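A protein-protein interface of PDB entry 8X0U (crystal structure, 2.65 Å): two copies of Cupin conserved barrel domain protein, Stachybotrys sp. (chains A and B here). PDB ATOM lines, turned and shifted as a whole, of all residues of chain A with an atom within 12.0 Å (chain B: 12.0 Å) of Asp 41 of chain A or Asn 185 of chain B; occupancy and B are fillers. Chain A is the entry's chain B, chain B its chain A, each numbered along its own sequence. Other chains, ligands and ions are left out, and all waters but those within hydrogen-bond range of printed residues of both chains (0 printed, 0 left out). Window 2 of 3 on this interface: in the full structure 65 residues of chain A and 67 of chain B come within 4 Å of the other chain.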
ATOM      1  N   THR A  37      11.990 -21.503   2.799  1.00  0.00           N
ATOM      2  CA  THR A  37      13.140 -21.790   1.956  1.00  0.00           C
ATOM      3  C   THR A  37      14.427 -21.357   2.645  1.00  0.00           C
ATOM      4  O   THR A  37      14.420 -20.591   3.613  1.00  0.00           O
ATOM      5  CB  THR A  37      13.018 -21.091   0.598  1.00  0.00           C
ATOM      6  OG1 THR A  37      13.265 -19.689   0.756  1.00  0.00           O
ATOM      7  CG2 THR A  37      11.632 -21.298   0.011  1.00  0.00           C
ATOM      8  N   GLY A  38      15.537 -21.868   2.131  1.00  0.00           N
ATOM      9  CA  GLY A  38      16.834 -21.542   2.680  1.00  0.00           C
ATOM     10  C   GLY A  38      17.935 -22.096   1.807  1.00  0.00           C
ATOM     11  O   GLY A  38      17.701 -22.538   0.681  1.00  0.00           O
ATOM     12  N   HIS A  39      19.150 -22.072   2.347  1.00  0.00           N
ATOM     13  CA  HIS A  39      20.332 -22.518   1.630  1.00  0.00           C
ATOM     14  C   HIS A  39      20.930 -23.746   2.302  1.00  0.00           C
ATOM     15  O   HIS A  39      20.980 -23.832   3.533  1.00  0.00           O
ATOM     16  CB  HIS A  39      21.380 -21.407   1.559  1.00  0.00           C
ATOM     17  CG  HIS A  39      21.011 -20.287   0.640  1.00  0.00           C
ATOM     18  ND1 HIS A  39      20.097 -19.311   0.981  1.00  0.00           N
ATOM     19  CD2 HIS A  39      21.429 -19.989  -0.614  1.00  0.00           C
ATOM     20  CE1 HIS A  39      19.973 -18.459  -0.019  1.00  0.00           C
ATOM     21  NE2 HIS A  39      20.771 -18.846  -0.998  1.00  0.00           N
ATOM     22  N   ASP A  40      21.383 -24.693   1.484  1.00  0.00           N
ATOM     23  CA  ASP A  40      22.102 -25.853   1.984  1.00  0.00           C
ATOM     24  C   ASP A  40      23.582 -25.496   2.132  1.00  0.00           C
ATOM     25  O   ASP A  40      23.975 -24.331   2.029  1.00  0.00           O
ATOM     26  CB  ASP A  40      21.857 -27.062   1.076  1.00  0.00           C
ATOM     27  CG  ASP A  40      22.523 -26.937  -0.291  1.00  0.00           C
ATOM     28  OD1 ASP A  40      23.061 -25.860  -0.625  1.00  0.00           O
ATOM     29  OD2 ASP A  40      22.499 -27.936  -1.043  1.00  0.00           O
ATOM     30  N   ASP A  41      24.426 -26.500   2.376  1.00  0.00           N
ATOM     31  CA  ASP A  41      25.838 -26.232   2.619  1.00  0.00           C
ATOM     32  C   ASP A  41      26.587 -25.824   1.355  1.00  0.00           C
ATOM     33  O   ASP A  41      27.666 -25.229   1.458  1.00  0.00           O
ATOM     34  CB  ASP A  41      26.500 -27.458   3.249  1.00  0.00           C
ATOM     35  CG  ASP A  41      26.016 -27.718   4.665  1.00  0.00           C
ATOM     36  OD1 ASP A  41      25.594 -26.751   5.337  1.00  0.00           O
ATOM     37  OD2 ASP A  41      26.056 -28.885   5.108  1.00  0.00           O
ATOM     38  N   ASN A  42      26.045 -26.118   0.175  1.00  0.00           N
ATOM     39  CA  ASN A  42      26.712 -25.810  -1.084  1.00  0.00           C
ATOM     40  C   ASN A  42      26.277 -24.479  -1.683  1.00  0.00           C
ATOM     41  O   ASN A  42      26.786 -24.103  -2.745  1.00  0.00           O
ATOM     42  CB  ASN A  42      26.464 -26.927  -2.102  1.00  0.00           C
ATOM     43  CG  ASN A  42      26.715 -28.306  -1.530  1.00  0.00           C
ATOM     44  OD1 ASN A  42      25.845 -29.175  -1.568  1.00  0.00           O
ATOM     45  ND2 ASN A  42      27.913 -28.515  -0.992  1.00  0.00           N
ATOM     46  N   GLY A  43      25.363 -23.761  -1.038  1.00  0.00           N
ATOM     47  CA  GLY A  43      24.855 -22.522  -1.589  1.00  0.00           C
ATOM     48  C   GLY A  43      23.660 -22.674  -2.500  1.00  0.00           C
ATOM     49  O   GLY A  43      23.379 -21.760  -3.286  1.00  0.00           O
ATOM     50  N   LYS A  44      22.953 -23.796  -2.428  1.00  0.00           N
ATOM     51  CA  LYS A  44      21.776 -24.046  -3.247  1.00  0.00           C
ATOM     52  C   LYS A  44      20.517 -23.724  -2.457  1.00  0.00           C
ATOM     53  O   LYS A  44      20.453 -23.954  -1.246  1.00  0.00           O
ATOM     54  CB  LYS A  44      21.740 -25.502  -3.719  1.00  0.00           C
ATOM     55  CG  LYS A  44      22.912 -25.901  -4.597  1.00  0.00           C
ATOM     56  CD  LYS A  44      22.817 -25.247  -5.965  1.00  0.00           C
ATOM     57  CE  LYS A  44      23.854 -25.814  -6.921  1.00  0.00           C
ATOM     58  NZ  LYS A  44      23.643 -25.323  -8.311  1.00  0.00           N
ATOM     59  N   SER A  45      19.513 -23.190  -3.148  1.00  0.00           N
ATOM     60  CA  SER A  45      18.247 -22.840  -2.517  1.00  0.00           C
ATOM     61  C   SER A  45      17.384 -24.090  -2.381  1.00  0.00           C
ATOM     62  O   SER A  45      17.067 -24.745  -3.381  1.00  0.00           O
ATOM     63  CB  SER A  45      17.529 -21.767  -3.329  1.00  0.00           C
ATOM     64  OG  SER A  45      18.212 -20.529  -3.244  1.00  0.00           O
ATOM     65  N   VAL A  46      16.999 -24.416  -1.148  1.00  0.00           N
ATOM     66  CA  VAL A  46      16.260 -25.634  -0.841  1.00  0.00           C
ATOM     67  C   VAL A  46      15.129 -25.296   0.120  1.00  0.00           C
ATOM     68  O   VAL A  46      15.101 -24.230   0.739  1.00  0.00           O
ATOM     69  CB  VAL A  46      17.164 -26.730  -0.239  1.00  0.00           C
ATOM     70  CG1 VAL A  46      18.193 -27.194  -1.257  1.00  0.00           C
ATOM     71  CG2 VAL A  46      17.847 -26.217   1.022  1.00  0.00           C
ATOM     72  N   PHE A  47      14.188 -26.229   0.242  1.00  0.00           N
ATOM     73  CA  PHE A  47      13.062 -26.085   1.158  1.00  0.00           C
ATOM     74  C   PHE A  47      13.458 -26.652   2.514  1.00  0.00           C
ATOM     75  O   PHE A  47      13.804 -27.833   2.622  1.00  0.00           O
ATOM     76  CB  PHE A  47      11.821 -26.793   0.617  1.00  0.00           C
ATOM     77  CG  PHE A  47      11.163 -26.068  -0.518  1.00  0.00           C
ATOM     78  CD1 PHE A  47      10.266 -25.041  -0.271  1.00  0.00           C
ATOM     79  CD2 PHE A  47      11.441 -26.406  -1.830  1.00  0.00           C
ATOM     80  CE1 PHE A  47       9.662 -24.364  -1.311  1.00  0.00           C
ATOM     81  CE2 PHE A  47      10.838 -25.733  -2.875  1.00  0.00           C
ATOM     82  CZ  PHE A  47       9.946 -24.709  -2.614  1.00  0.00           C
ATOM     83  N   LEU A  48      13.407 -25.809   3.543  1.00  0.00           N
ATOM     84  CA  LEU A  48      13.826 -26.233   4.872  1.00  0.00           C
ATOM     85  C   LEU A  48      12.705 -26.945   5.617  1.00  0.00           C
ATOM     86  O   LEU A  48      12.958 -27.922   6.330  1.00  0.00           O
ATOM     87  CB  LEU A  48      14.320 -25.027   5.670  1.00  0.00           C
ATOM     88  CG  LEU A  48      15.566 -24.365   5.087  1.00  0.00           C
ATOM     89  CD1 LEU A  48      15.836 -23.035   5.756  1.00  0.00           C
ATOM     90  CD2 LEU A  48      16.762 -25.290   5.229  1.00  0.00           C
ATOM     91  N   GLN A  78      18.516 -10.743   9.837  1.00  0.00           N
ATOM     92  CA  GLN A  78      19.713 -11.567   9.730  1.00  0.00           C
ATOM     93  C   GLN A  78      19.303 -12.996   9.392  1.00  0.00           C
ATOM     94  O   GLN A  78      18.514 -13.607  10.121  1.00  0.00           O
ATOM     95  CB  GLN A  78      20.517 -11.528  11.029  1.00  0.00           C
ATOM     96  CG  GLN A  78      21.764 -12.391  11.005  1.00  0.00           C
ATOM     97  CD  GLN A  78      22.729 -11.983   9.911  1.00  0.00           C
ATOM     98  OE1 GLN A  78      23.138 -12.801   9.090  1.00  0.00           O
ATOM     99  NE2 GLN A  78      23.099 -10.707   9.896  1.00  0.00           N
ATOM    100  N   LEU A  79      19.836 -13.525   8.289  1.00  0.00           N
ATOM    101  CA  LEU A  79      19.475 -14.859   7.823  1.00  0.00           C
ATOM    102  C   LEU A  79      20.611 -15.868   7.888  1.00  0.00           C
ATOM    103  O   LEU A  79      20.346 -17.071   7.805  1.00  0.00           O
ATOM    104  CB  LEU A  79      18.967 -14.805   6.374  1.00  0.00           C
ATOM    105  CG  LEU A  79      17.821 -13.865   6.008  1.00  0.00           C
ATOM    106  CD1 LEU A  79      17.628 -13.845   4.500  1.00  0.00           C
ATOM    107  CD2 LEU A  79      16.540 -14.290   6.701  1.00  0.00           C
ATOM    108  N   ASN A  80      21.856 -15.420   8.023  1.00  0.00           N
ATOM    109  CA  ASN A  80      22.982 -16.342   7.987  1.00  0.00           C
ATOM    110  C   ASN A  80      23.024 -17.180   9.257  1.00  0.00           C
ATOM    111  O   ASN A  80      22.796 -16.681  10.361  1.00  0.00           O
ATOM    112  CB  ASN A  80      24.290 -15.576   7.806  1.00  0.00           C
ATOM    113  CG  ASN A  80      24.353 -14.841   6.484  1.00  0.00           C
ATOM    114  OD1 ASN A  80      24.574 -15.447   5.435  1.00  0.00           O
ATOM    115  ND2 ASN A  80      24.145 -13.530   6.522  1.00  0.00           N
ATOM    116  N   GLY A  81      23.318 -18.468   9.091  1.00  0.00           N
ATOM    117  CA  GLY A  81      23.240 -19.392  10.202  1.00  0.00           C
ATOM    118  C   GLY A  81      21.838 -19.705  10.666  1.00  0.00           C
ATOM    119  O   GLY A  81      21.676 -20.313  11.729  1.00  0.00           O
ATOM    120  N   ASN A  82      20.818 -19.295   9.907  1.00  0.00           N
ATOM    121  CA  ASN A  82      19.417 -19.586  10.210  1.00  0.00           C
ATOM    122  C   ASN A  82      18.990 -19.019  11.561  1.00  0.00           C
ATOM    123  O   ASN A  82      18.133 -19.590  12.241  1.00  0.00           O
ATOM    124  CB  ASN A  82      19.135 -21.091  10.151  1.00  0.00           C
ATOM    125  CG  ASN A  82      19.229 -21.644   8.743  1.00  0.00           C
ATOM    126  OD1 ASN A  82      19.111 -20.905   7.766  1.00  0.00           O
ATOM    127  ND2 ASN A  82      19.441 -22.950   8.634  1.00  0.00           N
ATOM    128  N   ARG B 118      17.055 -14.025  -7.933  1.00  0.00           N
ATOM    129  CA  ARG B 118      17.253 -13.919  -6.494  1.00  0.00           C
ATOM    130  C   ARG B 118      17.185 -12.457  -6.094  1.00  0.00           C
ATOM    131  O   ARG B 118      18.032 -11.658  -6.505  1.00  0.00           O
ATOM    132  CB  ARG B 118      18.591 -14.522  -6.057  1.00  0.00           C
ATOM    133  CG  ARG B 118      18.840 -14.376  -4.566  1.00  0.00           C
ATOM    134  CD  ARG B 118      20.317 -14.416  -4.218  1.00  0.00           C
ATOM    135  NE  ARG B 118      20.976 -15.621  -4.711  1.00  0.00           N
ATOM    136  CZ  ARG B 118      20.861 -16.815  -4.142  1.00  0.00           C
ATOM    137  NH1 ARG B 118      20.099 -16.965  -3.068  1.00  0.00           N
ATOM    138  NH2 ARG B 118      21.500 -17.858  -4.653  1.00  0.00           N
ATOM    139  N   ASP B 137      16.504 -23.030  -7.254  1.00  0.00           N
ATOM    140  CA  ASP B 137      17.618 -23.227  -8.177  1.00  0.00           C
ATOM    141  C   ASP B 137      18.150 -24.655  -8.155  1.00  0.00           C
ATOM    142  O   ASP B 137      18.791 -25.081  -9.123  1.00  0.00           O
ATOM    143  CB  ASP B 137      18.745 -22.220  -7.883  1.00  0.00           C
ATOM    144  CG  ASP B 137      19.478 -22.489  -6.566  1.00  0.00           C
ATOM    145  OD1 ASP B 137      19.144 -23.453  -5.842  1.00  0.00           O
ATOM    146  OD2 ASP B 137      20.411 -21.715  -6.252  1.00  0.00           O
ATOM    147  N   SER B 138      17.900 -25.400  -7.078  1.00  0.00           N
ATOM    148  CA  SER B 138      18.325 -26.789  -6.986  1.00  0.00           C
ATOM    149  C   SER B 138      17.375 -27.750  -7.687  1.00  0.00           C
ATOM    150  O   SER B 138      17.719 -28.926  -7.852  1.00  0.00           O
ATOM    151  CB  SER B 138      18.464 -27.195  -5.517  1.00  0.00           C
ATOM    152  OG  SER B 138      17.329 -26.791  -4.769  1.00  0.00           O
ATOM    153  N   GLU B 140      14.273 -28.384  -6.451  1.00  0.00           N
ATOM    154  CA  GLU B 140      13.194 -28.650  -5.511  1.00  0.00           C
ATOM    155  C   GLU B 140      11.985 -27.788  -5.854  1.00  0.00           C
ATOM    156  O   GLU B 140      12.113 -26.681  -6.381  1.00  0.00           O
ATOM    157  CB  GLU B 140      13.655 -28.374  -4.079  1.00  0.00           C
ATOM    158  CG  GLU B 140      14.920 -29.115  -3.681  1.00  0.00           C
ATOM    159  CD  GLU B 140      15.132 -29.154  -2.177  1.00  0.00           C
ATOM    160  OE1 GLU B 140      15.964 -29.964  -1.717  1.00  0.00           O
ATOM    161  OE2 GLU B 140      14.470 -28.378  -1.455  1.00  0.00           O
ATOM    162  N   ARG B 153      13.446 -16.778   1.943  1.00  0.00           N
ATOM    163  CA  ARG B 153      14.577 -16.219   2.682  1.00  0.00           C
ATOM    164  C   ARG B 153      15.769 -16.017   1.747  1.00  0.00           C
ATOM    165  O   ARG B 153      16.755 -16.756   1.764  1.00  0.00           O
ATOM    166  CB  ARG B 153      14.926 -17.118   3.864  1.00  0.00           C
ATOM    167  CG  ARG B 153      13.814 -17.210   4.896  1.00  0.00           C
ATOM    168  CD  ARG B 153      14.085 -18.303   5.919  1.00  0.00           C
ATOM    169  NE  ARG B 153      15.274 -18.029   6.721  1.00  0.00           N
ATOM    170  CZ  ARG B 153      16.437 -18.655   6.572  1.00  0.00           C
ATOM    171  NH1 ARG B 153      16.569 -19.596   5.647  1.00  0.00           N
ATOM    172  NH2 ARG B 153      17.469 -18.340   7.345  1.00  0.00           N
ATOM    173  N   THR B 155      16.379 -16.568  -1.248  1.00  0.00           N
ATOM    174  CA  THR B 155      16.740 -17.714  -2.066  1.00  0.00           C
ATOM    175  C   THR B 155      16.452 -17.437  -3.538  1.00  0.00           C
ATOM    176  O   THR B 155      15.625 -16.591  -3.888  1.00  0.00           O
ATOM    177  CB  THR B 155      15.976 -18.959  -1.608  1.00  0.00           C
ATOM    178  OG1 THR B 155      14.569 -18.689  -1.617  1.00  0.00           O
ATOM    179  CG2 THR B 155      16.400 -19.355  -0.203  1.00  0.00           C
ATOM    180  N   ASP B 181      22.833  -9.499   3.551  1.00  0.00           N
ATOM    181  CA  ASP B 181      23.318 -10.376   2.494  1.00  0.00           C
ATOM    182  C   ASP B 181      23.553 -11.783   3.030  1.00  0.00           C
ATOM    183  O   ASP B 181      24.052 -11.969   4.143  1.00  0.00           O
ATOM    184  CB  ASP B 181      24.604  -9.816   1.890  1.00  0.00           C
ATOM    185  CG  ASP B 181      24.340  -8.767   0.829  1.00  0.00           C
ATOM    186  OD1 ASP B 181      23.618  -9.073  -0.144  1.00  0.00           O
ATOM    187  OD2 ASP B 181      24.854  -7.637   0.973  1.00  0.00           O
ATOM    188  N   VAL B 182      23.179 -12.777   2.232  1.00  0.00           N
ATOM    189  CA  VAL B 182      23.368 -14.179   2.586  1.00  0.00           C
ATOM    190  C   VAL B 182      24.779 -14.589   2.181  1.00  0.00           C
ATOM    191  O   VAL B 182      25.167 -14.442   1.017  1.00  0.00           O
ATOM    192  CB  VAL B 182      22.317 -15.072   1.909  1.00  0.00           C
ATOM    193  CG1 VAL B 182      22.755 -16.528   1.938  1.00  0.00           C
ATOM    194  CG2 VAL B 182      20.967 -14.905   2.585  1.00  0.00           C
ATOM    195  N   VAL B 183      25.545 -15.106   3.138  1.00  0.00           N
ATOM    196  CA  VAL B 183      26.924 -15.523   2.914  1.00  0.00           C
ATOM    197  C   VAL B 183      27.047 -16.990   3.303  1.00  0.00           C
ATOM    198  O   VAL B 183      26.830 -17.349   4.467  1.00  0.00           O
ATOM    199  CB  VAL B 183      27.922 -14.663   3.705  1.00  0.00           C
ATOM    200  CG1 VAL B 183      29.347 -15.124   3.432  1.00  0.00           C
ATOM    201  CG2 VAL B 183      27.757 -13.192   3.350  1.00  0.00           C
ATOM    202  N   VAL B 184      27.393 -17.832   2.333  1.00  0.00           N
ATOM    203  CA  VAL B 184      27.585 -19.262   2.549  1.00  0.00           C
ATOM    204  C   VAL B 184      29.067 -19.562   2.362  1.00  0.00           C
ATOM    205  O   VAL B 184      29.584 -19.502   1.240  1.00  0.00           O
ATOM    206  CB  VAL B 184      26.717 -20.106   1.604  1.00  0.00           C
ATOM    207  CG1 VAL B 184      27.241 -21.535   1.519  1.00  0.00           C
ATOM    208  CG2 VAL B 184      25.270 -20.098   2.072  1.00  0.00           C
ATOM    209  N   ASN B 185      29.747 -19.871   3.464  1.00  0.00           N
ATOM    210  CA  ASN B 185      31.146 -20.297   3.469  1.00  0.00           C
ATOM    211  C   ASN B 185      32.035 -19.287   2.743  1.00  0.00           C
ATOM    212  O   ASN B 185      32.748 -19.604   1.790  1.00  0.00           O
ATOM    213  CB  ASN B 185      31.289 -21.694   2.862  1.00  0.00           C
ATOM    214  CG  ASN B 185      30.843 -22.785   3.813  1.00  0.00           C
ATOM    215  OD1 ASN B 185      31.007 -22.660   5.028  1.00  0.00           O
ATOM    216  ND2 ASN B 185      30.274 -23.857   3.274  1.00  0.00           N
ATOM    217  N   GLY B 186      31.970 -18.042   3.216  1.00  0.00           N
ATOM    218  CA  GLY B 186      32.717 -16.955   2.624  1.00  0.00           C
ATOM    219  C   GLY B 186      32.115 -16.367   1.366  1.00  0.00           C
ATOM    220  O   GLY B 186      32.440 -15.227   1.019  1.00  0.00           O
ATOM    221  N   GLN B 187      31.246 -17.097   0.672  1.00  0.00           N
ATOM    222  CA  GLN B 187      30.688 -16.646  -0.598  1.00  0.00           C
ATOM    223  C   GLN B 187      29.393 -15.876  -0.359  1.00  0.00           C
ATOM    224  O   GLN B 187      28.556 -16.293   0.445  1.00  0.00           O
ATOM    225  CB  GLN B 187      30.423 -17.843  -1.516  1.00  0.00           C
ATOM    226  CG  GLN B 187      31.417 -18.968  -1.355  1.00  0.00           C
ATOM    227  CD  GLN B 187      31.252 -20.037  -2.411  1.00  0.00           C
ATOM    228  OE1 GLN B 187      30.254 -20.068  -3.137  1.00  0.00           O
ATOM    229  NE2 GLN B 187      32.233 -20.920  -2.505  1.00  0.00           N
ATOM    230  N   VAL B 188      29.234 -14.758  -1.058  1.00  0.00           N
ATOM    231  CA  VAL B 188      28.002 -13.978  -1.006  1.00  0.00           C
ATOM    232  C   VAL B 188      27.058 -14.491  -2.086  1.00  0.00           C
ATOM    233  O   VAL B 188      27.408 -14.510  -3.272  1.00  0.00           O
ATOM    234  CB  VAL B 188      28.285 -12.480  -1.192  1.00  0.00           C
ATOM    235  CG1 VAL B 188      26.985 -11.710  -1.374  1.00  0.00           C
ATOM    236  CG2 VAL B 188      29.068 -11.934  -0.009  1.00  0.00           C
ATOM    237  N   MET B 189      25.864 -14.915  -1.678  1.00  0.00           N
ATOM    238  CA  MET B 189      24.802 -15.250  -2.627  1.00  0.00           C
ATOM    239  C   MET B 189      24.251 -13.934  -3.155  1.00  0.00           C
ATOM    240  O   MET B 189      23.414 -13.295  -2.514  1.00  0.00           O
ATOM    241  CB  MET B 189      23.716 -16.086  -1.961  1.00  0.00           C
ATOM    242  CG  MET B 189      24.193 -17.424  -1.417  1.00  0.00           C
ATOM    243  SD  MET B 189      25.135 -18.387  -2.617  1.00  0.00           S
ATOM    244  CE  MET B 189      26.750 -18.414  -1.841  1.00  0.00           C
ATOM    245  N   GLU B 190      24.727 -13.519  -4.324  1.00  0.00           N
ATOM    246  CA  GLU B 190      24.435 -12.190  -4.839  1.00  0.00           C
ATOM    247  C   GLU B 190      23.094 -12.161  -5.555  1.00  0.00           C
ATOM    248  O   GLU B 190      22.708 -13.125  -6.224  1.00  0.00           O
ATOM    249  CB  GLU B 190      25.544 -11.726  -5.784  1.00  0.00           C
ATOM    250  CG  GLU B 190      26.770 -11.197  -5.062  1.00  0.00           C
ATOM    251  CD  GLU B 190      28.032 -11.307  -5.891  1.00  0.00           C
ATOM    252  OE1 GLU B 190      28.965 -12.016  -5.457  1.00  0.00           O
ATOM    253  OE2 GLU B 190      28.092 -10.680  -6.970  1.00  0.00           O
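NE2 of His 39 of chain A lies within hydrogen-bond range of NH1 of Arg 118 of chain B, at 2.9 Å. N of Ser 45 of chain A lies within hydrogen-bond range of OD1 of Asp 137 of chain B, 2.7 Å away. The side-chain hydroxyl (OG) of Ser 138 of chain B sits at hydrogen-bond distance from the backbone carbonyl oxygen (O) of Ser 45 of chain A, 2.5 Å away. OE2 of Glu 140 of chain B sits at hydrogen-bond distance from N of Phe 47 of chain A (2.8 Å). The backbone carbonyl oxygen (O) of Thr 37 of chain A sits at hydrogen-bond distance from the guanidinium group (NH1) of Arg 153 of chain B (3.1 Å). NH2 of Arg 153 of chain B lies within hydrogen-bond range of O of Leu 79 of chain A, 3.2 Å away. OD1 of Asn 82 of chain A sits at hydrogen-bond distance from NH2 of Arg 153 of chain B. The side-chain hydroxyl (OG1) of Thr 37 of chain A is in hydrogen-bond range of the side-chain hydroxyl (OG1) of Thr 155 of chain B, at 2.9 Å. O of Asp 181 of chain B sits at hydrogen-bond distance from ND2 of Asn 80 of chain A (2.8 Å). N of Val 183 of chain B sits at hydrogen-bond distance from OD1 of Asn 80 of chain A. The side-chain amide nitrogen of Asn 185 of chain B lies within hydrogen-bond range of the backbone carbonyl oxygen of Asp 41 of chain A (3.5 Å).
NE of Arg 118 of chain B sits close to O of Glu 190 of chain B (3.4 Å). The backbone NH (N) of Met 189 of chain B lies within hydrogen-bond range of the backbone carbonyl oxygen (O) of Val 182 of chain B (2.8 Å). O of Gly 38 of chain A lies within hydrogen-bond range of N of Val 46 of chain A (2.7 Å). N of Gly 43 of chain A lies within hydrogen-bond range of OD1 of Asp 40 of chain A (3.1 Å). The side-chain carboxylate of Asp 40 of chain A sits at hydrogen-bond distance from the backbone NH of Lys 44 of chain A (2.7 Å). The side-chain amide oxygen of Gln 78 of chain A is in hydrogen-bond range of the side-chain amide nitrogen of Asn 80 of chain A (2.9 Å).
Among the printed residues, merely in contact across the chains: Ser 45 of chain A with Thr 155 of chain B (3.2 Å), Val 46 of chain A with Glu 140 of chain B (3.3 Å), Asn 80 of chain A with Val 182 of chain B (3.3 Å), Leu 48 of chain A with Arg 153 of chain B (3.5 Å), Gly 38 of chain A with Thr 155 of chain B (3.5 Å), Gly 38 of chain A with Arg 153 of chain B (3.6 Å), Val 46 of chain A with Ser 138 of chain B (3.6 Å), Lys 44 of chain A with Asp 137 of chain B (3.7 Å), His 39 of chain A with Thr 155 of chain B (3.7 Å), Asp 41 of chain A with Val 184 of chain B (3.7 Å), His 39 of chain A with Met 189 of chain B (3.7 Å), Gly 43 of chain A with Met 189 of chain B (3.9 Å), Gly 43 of chain A with Val 184 of chain B (3.9 Å), His 39 of chain A with Val 182 of chain B (3.9 Å) and Leu 79 of chain A with Val 182 of chain B (3.99 Å).
Asn 185 of chain B touches one residue of chain A. No residue of chain B comes within 4 Å of Asp 40 of chain A. Of chain B, only Val 184 (3.9 Å) and Met 189 (3.9 Å) come within 4 Å of Gly 43 of chain A. Val 183 of chain B touches just one residue of chain A: Asn 80 (2.5 Å). Of the printed residues of chain A, Val 184 of chain B touches Asp 41 and Gly 43. Gln 187 of chain B touches none of the printed residues of chain A. Printed residues of chain B within 4 Å of Phe 47 of chain A: Glu 140. Printed residues of chain A within 4 Å of Arg 153 of chain B: Thr 37 (3.1 Å), Gly 38 (3.6 Å), Leu 48 (3.5 Å), Leu 79 (3.2 Å) and Asn 82 (3.1 Å). Of the printed residues of chain A, Asp 181 of chain B touches Asn 80.
Printed residues of chain A that touch a printed residue of chain B: Thr 37, Gly 38, His 39, Asp 41, Gly 43, Lys 44, Ser 45, Val 46, Phe 47, Leu 48, Leu 79, Asn 80 and Asn 82. Hydrophobic or aromatic side chains of chain A that line the printed part of chain B: His 39, Val 46, Phe 47, Leu 48 and Leu 79. Of the 16 printed residues of chain B, 12 touch a printed residue of chain A. Hydrophobic or aromatic side chains of chain B within 4 Å of the printed part of chain A: Val 182, Val 183, Val 184 and Met 189. Among the printed residues, 26 pairs touch across the chains. Among the printed residues, no Asp or Glu carboxylate lies within 4 Å of a Lys or Arg side-chain nitrogen of the other chain.
No position is printed for both chains.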
